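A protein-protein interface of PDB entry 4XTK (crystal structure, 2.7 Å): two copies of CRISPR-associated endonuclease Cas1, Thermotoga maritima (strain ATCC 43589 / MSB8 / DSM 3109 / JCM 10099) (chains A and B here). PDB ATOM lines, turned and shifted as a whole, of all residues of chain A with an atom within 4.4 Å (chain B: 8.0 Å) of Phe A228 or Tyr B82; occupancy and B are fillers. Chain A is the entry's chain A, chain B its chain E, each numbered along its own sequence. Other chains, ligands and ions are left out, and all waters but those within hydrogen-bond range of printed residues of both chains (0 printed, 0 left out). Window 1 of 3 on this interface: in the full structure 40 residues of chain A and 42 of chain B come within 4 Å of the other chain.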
ATOM      1  N   GLY A  79     -28.959  17.668  23.149  1.00  0.00           N
ATOM      2  CA  GLY A  79     -28.876  17.024  21.854  1.00  0.00           C
ATOM      3  C   GLY A  79     -28.237  17.820  20.732  1.00  0.00           C
ATOM      4  O   GLY A  79     -27.815  18.962  20.907  1.00  0.00           O
ATOM      5  N   THR A  80     -28.185  17.206  19.557  1.00  0.00           N
ATOM      6  CA  THR A  80     -27.453  17.768  18.435  1.00  0.00           C
ATOM      7  C   THR A  80     -28.284  17.730  17.161  1.00  0.00           C
ATOM      8  O   THR A  80     -29.024  16.775  16.928  1.00  0.00           O
ATOM      9  CB  THR A  80     -26.134  16.998  18.207  1.00  0.00           C
ATOM     10  OG1 THR A  80     -25.304  17.113  19.369  1.00  0.00           O
ATOM     11  CG2 THR A  80     -25.383  17.532  16.988  1.00  0.00           C
ATOM     12  N   TYR A  82     -27.637  16.999  13.598  1.00  0.00           N
ATOM     13  CA  TYR A  82     -26.584  16.390  12.806  1.00  0.00           C
ATOM     14  C   TYR A  82     -26.961  16.490  11.340  1.00  0.00           C
ATOM     15  O   TYR A  82     -27.932  15.869  10.912  1.00  0.00           O
ATOM     16  CB  TYR A  82     -26.388  14.939  13.228  1.00  0.00           C
ATOM     17  CG  TYR A  82     -25.026  14.368  12.925  1.00  0.00           C
ATOM     18  CD1 TYR A  82     -23.899  14.790  13.622  1.00  0.00           C
ATOM     19  CD2 TYR A  82     -24.873  13.378  11.968  1.00  0.00           C
ATOM     20  CE1 TYR A  82     -22.654  14.261  13.351  1.00  0.00           C
ATOM     21  CE2 TYR A  82     -23.643  12.844  11.695  1.00  0.00           C
ATOM     22  CZ  TYR A  82     -22.536  13.284  12.382  1.00  0.00           C
ATOM     23  OH  TYR A  82     -21.311  12.735  12.084  1.00  0.00           O
ATOM     24  N   LEU A 205     -17.882  14.691  18.255  1.00  0.00           N
ATOM     25  CA  LEU A 205     -19.032  14.463  17.384  1.00  0.00           C
ATOM     26  C   LEU A 205     -18.975  15.311  16.114  1.00  0.00           C
ATOM     27  O   LEU A 205     -19.210  14.810  15.017  1.00  0.00           O
ATOM     28  CB  LEU A 205     -20.340  14.748  18.127  1.00  0.00           C
ATOM     29  CG  LEU A 205     -21.589  14.431  17.298  1.00  0.00           C
ATOM     30  CD1 LEU A 205     -21.565  12.970  16.870  1.00  0.00           C
ATOM     31  CD2 LEU A 205     -22.878  14.762  18.044  1.00  0.00           C
ATOM     32  N   PRO A 215     -21.234   8.231  13.386  1.00  0.00           N
ATOM     33  CA  PRO A 215     -21.124   8.409  14.838  1.00  0.00           C
ATOM     34  C   PRO A 215     -21.996   7.439  15.638  1.00  0.00           C
ATOM     35  O   PRO A 215     -21.802   7.313  16.844  1.00  0.00           O
ATOM     36  CB  PRO A 215     -21.596   9.849  15.044  1.00  0.00           C
ATOM     37  CG  PRO A 215     -22.564  10.071  13.934  1.00  0.00           C
ATOM     38  CD  PRO A 215     -21.992   9.326  12.757  1.00  0.00           C
ATOM     39  N   ARG A 216     -22.948   6.783  14.976  1.00  0.00           N
ATOM     40  CA  ARG A 216     -23.875   5.872  15.650  1.00  0.00           C
ATOM     41  C   ARG A 216     -23.283   4.492  15.907  1.00  0.00           C
ATOM     42  O   ARG A 216     -23.805   3.734  16.726  1.00  0.00           O
ATOM     43  CB  ARG A 216     -25.157   5.725  14.841  1.00  0.00           C
ATOM     44  CG  ARG A 216     -26.027   6.956  14.873  1.00  0.00           C
ATOM     45  CD  ARG A 216     -27.124   6.883  13.833  1.00  0.00           C
ATOM     46  NE  ARG A 216     -26.589   6.960  12.482  1.00  0.00           N
ATOM     47  CZ  ARG A 216     -27.340   6.985  11.386  1.00  0.00           C
ATOM     48  NH1 ARG A 216     -28.666   6.933  11.483  1.00  0.00           N
ATOM     49  NH2 ARG A 216     -26.765   7.057  10.192  1.00  0.00           N
ATOM     50  N   ARG A 227     -28.380   6.433  20.689  1.00  0.00           N
ATOM     51  CA  ARG A 227     -27.394   7.481  20.948  1.00  0.00           C
ATOM     52  C   ARG A 227     -26.219   7.423  19.977  1.00  0.00           C
ATOM     53  O   ARG A 227     -26.074   6.477  19.205  1.00  0.00           O
ATOM     54  CB  ARG A 227     -26.842   7.346  22.361  1.00  0.00           C
ATOM     55  CG  ARG A 227     -25.948   6.129  22.448  1.00  0.00           C
ATOM     56  CD  ARG A 227     -25.306   5.923  23.786  1.00  0.00           C
ATOM     57  NE  ARG A 227     -24.668   4.612  23.799  1.00  0.00           N
ATOM     58  CZ  ARG A 227     -24.030   4.096  24.841  1.00  0.00           C
ATOM     59  NH1 ARG A 227     -23.933   4.784  25.971  1.00  0.00           N
ATOM     60  NH2 ARG A 227     -23.490   2.889  24.748  1.00  0.00           N
ATOM     61  N   PHE A 228     -25.364   8.433  20.036  1.00  0.00           N
ATOM     62  CA  PHE A 228     -24.090   8.357  19.344  1.00  0.00           C
ATOM     63  C   PHE A 228     -23.101   7.639  20.250  1.00  0.00           C
ATOM     64  O   PHE A 228     -23.061   7.870  21.455  1.00  0.00           O
ATOM     65  CB  PHE A 228     -23.572   9.747  18.961  1.00  0.00           C
ATOM     66  CG  PHE A 228     -24.457  10.482  17.996  1.00  0.00           C
ATOM     67  CD1 PHE A 228     -24.713   9.963  16.738  1.00  0.00           C
ATOM     68  CD2 PHE A 228     -25.018  11.699  18.337  1.00  0.00           C
ATOM     69  CE1 PHE A 228     -25.522  10.635  15.848  1.00  0.00           C
ATOM     70  CE2 PHE A 228     -25.827  12.376  17.450  1.00  0.00           C
ATOM     71  CZ  PHE A 228     -26.077  11.845  16.202  1.00  0.00           C
ATOM     72  N   SER A 229     -22.310   6.759  19.660  1.00  0.00           N
ATOM     73  CA  SER A 229     -21.389   5.923  20.413  1.00  0.00           C
ATOM     74  C   SER A 229     -19.948   6.298  20.109  1.00  0.00           C
ATOM     75  O   SER A 229     -19.168   6.564  21.021  1.00  0.00           O
ATOM     76  CB  SER A 229     -21.637   4.445  20.129  1.00  0.00           C
ATOM     77  OG  SER A 229     -22.820   4.020  20.773  1.00  0.00           O
ATOM     78  N   LEU A 230     -19.588   6.251  18.830  1.00  0.00           N
ATOM     79  CA  LEU A 230     -18.219   6.493  18.397  1.00  0.00           C
ATOM     80  C   LEU A 230     -17.619   7.735  19.053  1.00  0.00           C
ATOM     81  O   LEU A 230     -16.440   7.741  19.402  1.00  0.00           O
ATOM     82  CB  LEU A 230     -18.151   6.624  16.871  1.00  0.00           C
ATOM     83  CG  LEU A 230     -16.736   6.603  16.282  1.00  0.00           C
ATOM     84  CD1 LEU A 230     -16.033   5.292  16.632  1.00  0.00           C
ATOM     85  CD2 LEU A 230     -16.749   6.823  14.774  1.00  0.00           C
ATOM     86  N   ASN A 231     -18.413   8.782  19.234  1.00  0.00           N
ATOM     87  CA  ASN A 231     -17.862   9.988  19.835  1.00  0.00           C
ATOM     88  C   ASN A 231     -17.562   9.774  21.320  1.00  0.00           C
ATOM     89  O   ASN A 231     -16.609  10.347  21.855  1.00  0.00           O
ATOM     90  CB  ASN A 231     -18.794  11.185  19.628  1.00  0.00           C
ATOM     91  CG  ASN A 231     -20.137  11.012  20.304  1.00  0.00           C
ATOM     92  OD1 ASN A 231     -20.736   9.935  20.264  1.00  0.00           O
ATOM     93  ND2 ASN A 231     -20.618  12.077  20.935  1.00  0.00           N
ATOM     94  N   LEU A 232     -18.354   8.929  21.974  1.00  0.00           N
ATOM     95  CA  LEU A 232     -18.098   8.566  23.365  1.00  0.00           C
ATOM     96  C   LEU A 232     -16.813   7.753  23.497  1.00  0.00           C
ATOM     97  O   LEU A 232     -16.030   7.964  24.417  1.00  0.00           O
ATOM     98  CB  LEU A 232     -19.271   7.779  23.941  1.00  0.00           C
ATOM     99  CG  LEU A 232     -20.610   8.512  23.971  1.00  0.00           C
ATOM    100  CD1 LEU A 232     -21.631   7.693  24.736  1.00  0.00           C
ATOM    101  CD2 LEU A 232     -20.458   9.902  24.579  1.00  0.00           C
ATOM    102  N   LEU B  58     -37.076  21.517  21.662  1.00  0.00           N
ATOM    103  CA  LEU B  58     -36.051  20.490  21.504  1.00  0.00           C
ATOM    104  C   LEU B  58     -35.773  19.803  22.842  1.00  0.00           C
ATOM    105  O   LEU B  58     -35.554  18.591  22.897  1.00  0.00           O
ATOM    106  CB  LEU B  58     -34.761  21.089  20.935  1.00  0.00           C
ATOM    107  CG  LEU B  58     -34.832  21.604  19.494  1.00  0.00           C
ATOM    108  CD1 LEU B  58     -33.459  22.056  18.990  1.00  0.00           C
ATOM    109  CD2 LEU B  58     -35.427  20.551  18.577  1.00  0.00           C
ATOM    110  N   LEU B  61     -38.657  17.222  23.251  1.00  0.00           N
ATOM    111  CA  LEU B  61     -38.379  16.039  22.442  1.00  0.00           C
ATOM    112  C   LEU B  61     -37.237  15.221  23.031  1.00  0.00           C
ATOM    113  O   LEU B  61     -37.278  13.992  23.036  1.00  0.00           O
ATOM    114  CB  LEU B  61     -38.038  16.431  21.005  1.00  0.00           C
ATOM    115  CG  LEU B  61     -39.166  16.964  20.122  1.00  0.00           C
ATOM    116  CD1 LEU B  61     -38.670  17.078  18.695  1.00  0.00           C
ATOM    117  CD2 LEU B  61     -40.384  16.071  20.200  1.00  0.00           C
ATOM    118  N   SER B  62     -36.224  15.919  23.530  1.00  0.00           N
ATOM    119  CA  SER B  62     -35.081  15.273  24.152  1.00  0.00           C
ATOM    120  C   SER B  62     -35.507  14.497  25.396  1.00  0.00           C
ATOM    121  O   SER B  62     -35.039  13.383  25.628  1.00  0.00           O
ATOM    122  CB  SER B  62     -34.017  16.313  24.504  1.00  0.00           C
ATOM    123  OG  SER B  62     -32.851  15.704  25.029  1.00  0.00           O
ATOM    124  N   ARG B  65     -37.228  11.562  24.348  1.00  0.00           N
ATOM    125  CA  ARG B  65     -36.305  10.721  23.596  1.00  0.00           C
ATOM    126  C   ARG B  65     -36.805  10.509  22.164  1.00  0.00           C
ATOM    127  O   ARG B  65     -36.678   9.424  21.591  1.00  0.00           O
ATOM    128  CB  ARG B  65     -36.095   9.398  24.334  1.00  0.00           C
ATOM    129  CG  ARG B  65     -35.499   9.621  25.724  1.00  0.00           C
ATOM    130  CD  ARG B  65     -35.381   8.361  26.572  1.00  0.00           C
ATOM    131  NE  ARG B  65     -34.689   8.665  27.825  1.00  0.00           N
ATOM    132  CZ  ARG B  65     -34.405   7.777  28.774  1.00  0.00           C
ATOM    133  NH1 ARG B  65     -34.748   6.505  28.629  1.00  0.00           N
ATOM    134  NH2 ARG B  65     -33.773   8.163  29.873  1.00  0.00           N
ATOM    135  N   ILE B  66     -37.364  11.578  21.601  1.00  0.00           N
ATOM    136  CA  ILE B  66     -37.905  11.583  20.247  1.00  0.00           C
ATOM    137  C   ILE B  66     -37.070  12.444  19.315  1.00  0.00           C
ATOM    138  O   ILE B  66     -37.056  13.670  19.448  1.00  0.00           O
ATOM    139  CB  ILE B  66     -39.348  12.119  20.219  1.00  0.00           C
ATOM    140  CG1 ILE B  66     -40.271  11.234  21.058  1.00  0.00           C
ATOM    141  CG2 ILE B  66     -39.837  12.256  18.789  1.00  0.00           C
ATOM    142  CD1 ILE B  66     -41.655  11.801  21.230  1.00  0.00           C
ATOM    143  N   PRO B  67     -36.380  11.814  18.356  1.00  0.00           N
ATOM    144  CA  PRO B  67     -35.640  12.615  17.385  1.00  0.00           C
ATOM    145  C   PRO B  67     -36.578  13.197  16.346  1.00  0.00           C
ATOM    146  O   PRO B  67     -37.677  12.676  16.128  1.00  0.00           O
ATOM    147  CB  PRO B  67     -34.665  11.611  16.763  1.00  0.00           C
ATOM    148  CG  PRO B  67     -35.202  10.256  17.100  1.00  0.00           C
ATOM    149  CD  PRO B  67     -36.415  10.400  17.972  1.00  0.00           C
ATOM    150  N   ILE B  68     -36.153  14.286  15.724  1.00  0.00           N
ATOM    151  CA  ILE B  68     -36.956  14.916  14.691  1.00  0.00           C
ATOM    152  C   ILE B  68     -36.104  15.079  13.438  1.00  0.00           C
ATOM    153  O   ILE B  68     -35.013  15.659  13.478  1.00  0.00           O
ATOM    154  CB  ILE B  68     -37.539  16.271  15.177  1.00  0.00           C
ATOM    155  CG1 ILE B  68     -38.290  16.987  14.061  1.00  0.00           C
ATOM    156  CG2 ILE B  68     -36.459  17.180  15.749  1.00  0.00           C
ATOM    157  CD1 ILE B  68     -39.067  18.174  14.571  1.00  0.00           C
ATOM    158  N   HIS B  69     -36.596  14.514  12.337  1.00  0.00           N
ATOM    159  CA  HIS B  69     -35.902  14.556  11.051  1.00  0.00           C
ATOM    160  C   HIS B  69     -36.431  15.694  10.181  1.00  0.00           C
ATOM    161  O   HIS B  69     -37.636  15.939  10.129  1.00  0.00           O
ATOM    162  CB  HIS B  69     -36.058  13.232  10.302  1.00  0.00           C
ATOM    163  CG  HIS B  69     -35.699  12.026  11.110  1.00  0.00           C
ATOM    164  ND1 HIS B  69     -34.398  11.712  11.439  1.00  0.00           N
ATOM    165  CD2 HIS B  69     -36.468  11.043  11.635  1.00  0.00           C
ATOM    166  CE1 HIS B  69     -34.383  10.595  12.146  1.00  0.00           C
ATOM    167  NE2 HIS B  69     -35.625  10.167  12.276  1.00  0.00           N
ATOM    168  N   PHE B  70     -35.526  16.376   9.487  1.00  0.00           N
ATOM    169  CA  PHE B  70     -35.908  17.512   8.659  1.00  0.00           C
ATOM    170  C   PHE B  70     -35.690  17.236   7.169  1.00  0.00           C
ATOM    171  O   PHE B  70     -34.657  16.694   6.768  1.00  0.00           O
ATOM    172  CB  PHE B  70     -35.130  18.763   9.091  1.00  0.00           C
ATOM    173  CG  PHE B  70     -35.463  19.232  10.479  1.00  0.00           C
ATOM    174  CD1 PHE B  70     -36.531  20.086  10.695  1.00  0.00           C
ATOM    175  CD2 PHE B  70     -34.715  18.814  11.568  1.00  0.00           C
ATOM    176  CE1 PHE B  70     -36.842  20.517  11.970  1.00  0.00           C
ATOM    177  CE2 PHE B  70     -35.022  19.243  12.846  1.00  0.00           C
ATOM    178  CZ  PHE B  70     -36.085  20.092  13.048  1.00  0.00           C
ATOM    179  N   TYR B  77     -33.437  14.991   2.388  1.00  0.00           N
ATOM    180  CA  TYR B  77     -33.112  14.982   3.801  1.00  0.00           C
ATOM    181  C   TYR B  77     -31.984  15.961   4.099  1.00  0.00           C
ATOM    182  O   TYR B  77     -30.904  15.866   3.517  1.00  0.00           O
ATOM    183  CB  TYR B  77     -32.745  13.555   4.205  1.00  0.00           C
ATOM    184  CG  TYR B  77     -32.133  13.406   5.565  1.00  0.00           C
ATOM    185  CD1 TYR B  77     -32.884  13.615   6.718  1.00  0.00           C
ATOM    186  CD2 TYR B  77     -30.809  13.026   5.703  1.00  0.00           C
ATOM    187  CE1 TYR B  77     -32.321  13.477   7.971  1.00  0.00           C
ATOM    188  CE2 TYR B  77     -30.238  12.881   6.947  1.00  0.00           C
ATOM    189  CZ  TYR B  77     -30.994  13.104   8.078  1.00  0.00           C
ATOM    190  OH  TYR B  77     -30.409  12.951   9.315  1.00  0.00           O
ATOM    191  N   GLY B  79     -31.133  16.844   7.510  1.00  0.00           N
ATOM    192  CA  GLY B  79     -30.525  16.503   8.787  1.00  0.00           C
ATOM    193  C   GLY B  79     -31.513  16.144   9.888  1.00  0.00           C
ATOM    194  O   GLY B  79     -32.726  16.226   9.710  1.00  0.00           O
ATOM    195  N   THR B  80     -30.983  15.748  11.039  1.00  0.00           N
ATOM    196  CA  THR B  80     -31.803  15.265  12.143  1.00  0.00           C
ATOM    197  C   THR B  80     -31.376  15.891  13.460  1.00  0.00           C
ATOM    198  O   THR B  80     -30.183  16.083  13.701  1.00  0.00           O
ATOM    199  CB  THR B  80     -31.719  13.721  12.269  1.00  0.00           C
ATOM    200  OG1 THR B  80     -32.301  13.104  11.113  1.00  0.00           O
ATOM    201  CG2 THR B  80     -32.430  13.217  13.525  1.00  0.00           C
ATOM    202  N   PHE B  81     -32.346  16.212  14.311  1.00  0.00           N
ATOM    203  CA  PHE B  81     -32.032  16.551  15.692  1.00  0.00           C
ATOM    204  C   PHE B  81     -32.082  15.276  16.524  1.00  0.00           C
ATOM    205  O   PHE B  81     -33.147  14.693  16.732  1.00  0.00           O
ATOM    206  CB  PHE B  81     -33.006  17.590  16.251  1.00  0.00           C
ATOM    207  CG  PHE B  81     -32.917  17.758  17.741  1.00  0.00           C
ATOM    208  CD1 PHE B  81     -31.928  18.546  18.306  1.00  0.00           C
ATOM    209  CD2 PHE B  81     -33.812  17.107  18.580  1.00  0.00           C
ATOM    210  CE1 PHE B  81     -31.837  18.688  19.680  1.00  0.00           C
ATOM    211  CE2 PHE B  81     -33.726  17.241  19.951  1.00  0.00           C
ATOM    212  CZ  PHE B  81     -32.739  18.034  20.503  1.00  0.00           C
ATOM    213  N   TYR B  82     -30.921  14.837  16.988  1.00  0.00           N
ATOM    214  CA  TYR B  82     -30.848  13.652  17.831  1.00  0.00           C
ATOM    215  C   TYR B  82     -30.749  14.065  19.289  1.00  0.00           C
ATOM    216  O   TYR B  82     -29.835  14.801  19.664  1.00  0.00           O
ATOM    217  CB  TYR B  82     -29.646  12.777  17.461  1.00  0.00           C
ATOM    218  CG  TYR B  82     -29.750  12.048  16.138  1.00  0.00           C
ATOM    219  CD1 TYR B  82     -30.449  10.850  16.029  1.00  0.00           C
ATOM    220  CD2 TYR B  82     -29.120  12.544  15.002  1.00  0.00           C
ATOM    221  CE1 TYR B  82     -30.532  10.177  14.819  1.00  0.00           C
ATOM    222  CE2 TYR B  82     -29.189  11.874  13.793  1.00  0.00           C
ATOM    223  CZ  TYR B  82     -29.899  10.696  13.703  1.00  0.00           C
ATOM    224  OH  TYR B  82     -29.968  10.041  12.493  1.00  0.00           O
ATOM    225  N   PRO B  83     -31.692  13.599  20.119  1.00  0.00           N
ATOM    226  CA  PRO B  83     -31.573  13.838  21.560  1.00  0.00           C
ATOM    227  C   PRO B  83     -30.359  13.097  22.093  1.00  0.00           C
ATOM    228  O   PRO B  83     -29.875  12.183  21.419  1.00  0.00           O
ATOM    229  CB  PRO B  83     -32.873  13.260  22.133  1.00  0.00           C
ATOM    230  CG  PRO B  83     -33.791  13.105  20.958  1.00  0.00           C
ATOM    231  CD  PRO B  83     -32.902  12.834  19.783  1.00  0.00           C
ATOM    232  N   ARG B  84     -29.877  13.492  23.264  1.00  0.00           N
ATOM    233  CA  ARG B  84     -28.772  12.809  23.919  1.00  0.00           C
ATOM    234  C   ARG B  84     -29.009  11.304  23.891  1.00  0.00           C
ATOM    235  O   ARG B  84     -28.207  10.561  23.335  1.00  0.00           O
ATOM    236  CB  ARG B  84     -28.599  13.322  25.349  1.00  0.00           C
ATOM    237  CG  ARG B  84     -27.470  12.677  26.118  1.00  0.00           C
ATOM    238  CD  ARG B  84     -27.344  13.332  27.476  1.00  0.00           C
ATOM    239  NE  ARG B  84     -26.632  12.515  28.450  1.00  0.00           N
ATOM    240  CZ  ARG B  84     -27.164  11.467  29.071  1.00  0.00           C
ATOM    241  NH1 ARG B  84     -28.412  11.106  28.808  1.00  0.00           N
ATOM    242  NH2 ARG B  84     -26.445  10.777  29.951  1.00  0.00           N
ATOM    243  N   GLU B  85     -30.096  10.847  24.499  1.00  0.00           N
ATOM    244  CA  GLU B  85     -30.560   9.491  24.242  1.00  0.00           C
ATOM    245  C   GLU B  85     -31.945   9.532  23.597  1.00  0.00           C
ATOM    246  O   GLU B  85     -32.770  10.380  23.921  1.00  0.00           O
ATOM    247  CB  GLU B  85     -30.580   8.639  25.521  1.00  0.00           C
ATOM    248  CG  GLU B  85     -31.349   7.322  25.344  1.00  0.00           C
ATOM    249  CD  GLU B  85     -30.957   6.231  26.327  1.00  0.00           C
ATOM    250  OE1 GLU B  85     -29.984   6.420  27.090  1.00  0.00           O
ATOM    251  OE2 GLU B  85     -31.617   5.169  26.316  1.00  0.00           O
ATOM    252  N   TYR B  86     -32.189   8.622  22.664  1.00  0.00           N
ATOM    253  CA  TYR B  86     -33.476   8.565  21.989  1.00  0.00           C
ATOM    254  C   TYR B  86     -33.980   7.129  21.901  1.00  0.00           C
ATOM    255  O   TYR B  86     -33.217   6.188  22.097  1.00  0.00           O
ATOM    256  CB  TYR B  86     -33.373   9.198  20.596  1.00  0.00           C
ATOM    257  CG  TYR B  86     -32.150   8.773  19.812  1.00  0.00           C
ATOM    258  CD1 TYR B  86     -32.168   7.633  19.021  1.00  0.00           C
ATOM    259  CD2 TYR B  86     -30.974   9.513  19.864  1.00  0.00           C
ATOM    260  CE1 TYR B  86     -31.056   7.242  18.302  1.00  0.00           C
ATOM    261  CE2 TYR B  86     -29.857   9.131  19.147  1.00  0.00           C
ATOM    262  CZ  TYR B  86     -29.901   7.992  18.371  1.00  0.00           C
ATOM    263  OH  TYR B  86     -28.793   7.597  17.654  1.00  0.00           O
ATOM    264  N   LEU B  87     -35.270   6.975  21.621  1.00  0.00           N
ATOM    265  CA  LEU B  87     -35.884   5.664  21.439  1.00  0.00           C
ATOM    266  C   LEU B  87     -35.164   4.880  20.350  1.00  0.00           C
ATOM    267  O   LEU B  87     -34.643   5.475  19.406  1.00  0.00           O
ATOM    268  CB  LEU B  87     -37.358   5.814  21.076  1.00  0.00           C
ATOM    269  CG  LEU B  87     -38.216   6.567  22.090  1.00  0.00           C
ATOM    270  CD1 LEU B  87     -39.561   6.914  21.484  1.00  0.00           C
ATOM    271  CD2 LEU B  87     -38.393   5.740  23.344  1.00  0.00           C
ATOM    272  N   SER B  89     -34.026   3.335  17.212  1.00  0.00           N
ATOM    273  CA  SER B  89     -34.385   3.896  15.914  1.00  0.00           C
ATOM    274  C   SER B  89     -34.631   2.816  14.875  1.00  0.00           C
ATOM    275  O   SER B  89     -35.114   3.104  13.782  1.00  0.00           O
ATOM    276  CB  SER B  89     -33.294   4.835  15.416  1.00  0.00           C
ATOM    277  OG  SER B  89     -32.167   4.094  14.988  1.00  0.00           O
ATOM    278  N   PHE B  91     -32.541   1.420  13.162  1.00  0.00           N
ATOM    279  CA  PHE B  91     -31.570   1.606  12.096  1.00  0.00           C
ATOM    280  C   PHE B  91     -30.957   0.259  11.699  1.00  0.00           C
ATOM    281  O   PHE B  91     -30.488  -0.504  12.546  1.00  0.00           O
ATOM    282  CB  PHE B  91     -30.505   2.607  12.557  1.00  0.00           C
ATOM    283  CG  PHE B  91     -29.574   3.045  11.482  1.00  0.00           C
ATOM    284  CD1 PHE B  91     -30.024   3.211  10.186  1.00  0.00           C
ATOM    285  CD2 PHE B  91     -28.256   3.342  11.774  1.00  0.00           C
ATOM    286  CE1 PHE B  91     -29.164   3.628   9.185  1.00  0.00           C
ATOM    287  CE2 PHE B  91     -27.393   3.763  10.785  1.00  0.00           C
ATOM    288  CZ  PHE B  91     -27.847   3.907   9.486  1.00  0.00           C
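The backbone carbonyl oxygen (O) of Thr B80 lies close to the backbone carbonyl oxygen (O) of Thr A80, at 3.5 Å. The backbone NH (N) of Tyr A82 is in hydrogen-bond range of the backbone carbonyl oxygen (O) of Thr B80. N of Arg A227 sits close to OH of Tyr B86, 3.3 Å away. The backbone carbonyl oxygen of Thr A80 lies within hydrogen-bond range of the backbone NH of Tyr B82 (2.7 Å).
The backbone NH (N) of Phe B81 is in hydrogen-bond range of the backbone carbonyl oxygen (O) of Ile B68, 2.8 Å away. The side-chain hydroxyl of Tyr B77 sits at hydrogen-bond distance from the side-chain hydroxyl of Thr B80. The backbone carbonyl oxygen (O) of Phe A228 sits close to the side-chain amide oxygen (OD1) of Asn A231 (3.3 Å). The backbone carbonyl oxygen (O) of Gly B79 sits at hydrogen-bond distance from the backbone NH (N) of Phe B70 (2.8 Å). A ring nitrogen (ND1) of His B69 sits at hydrogen-bond distance from the side-chain hydroxyl (OG1) of Thr B80, 2.5 Å away. OG of Ser B89 sits close to N of Phe B91, 3.3 Å away.
Gly A79 touches Phe B81. Gly A79 touches Tyr B82 (CA to O, 3.3 Å). Arg B84 touches Gly A79 (N to CA, 3.9 Å). Thr A80 touches Phe B81 (O to CA, 3.3 Å). O of Tyr A82 touches CA of Gly B79 (3.4 Å). Arg A216 touches Tyr B82 (NH1 to OH, 3.5 Å). Tyr B86 touches Arg A216. Arg A216 touches Phe B91 (CZ to CE2, 3.3 Å). Arg A227 touches Arg B84 (CB to O, 3.6 Å). Phe A228 touches Tyr B82.
Printed residues of chain B within 4 Å of Arg A227: Arg B84 and Tyr B86. Phe A228 touches just one residue of chain B: Tyr B82. Of chain A, only Gly A79, Thr A80, Arg A216 and Phe A228 come within 4 Å of Tyr B82. Leu B87 touches none of the printed residues of chain A. Of the printed residues of chain A, Phe B91 touches Arg A216 (3.3 Å).
Printed residues of chain A that touch a printed residue of chain B: Gly A79, Thr A80, Tyr A82, Arg A216, Arg A227 and Phe A228. Among the printed residues, 14 pairs touch across the chains. Among the printed residues, no Asp or Glu carboxylate lies within 4 Å of a Lys or Arg side-chain nitrogen of the other chain.
Gly A79 touches Tyr B82, and with the chains exchanged Tyr A82 touches Gly B79. Thr B80 touches its own counterpart, Thr A80. Thr A80 touches Tyr B82, and with the chains exchanged Tyr A82 touches Thr B80.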
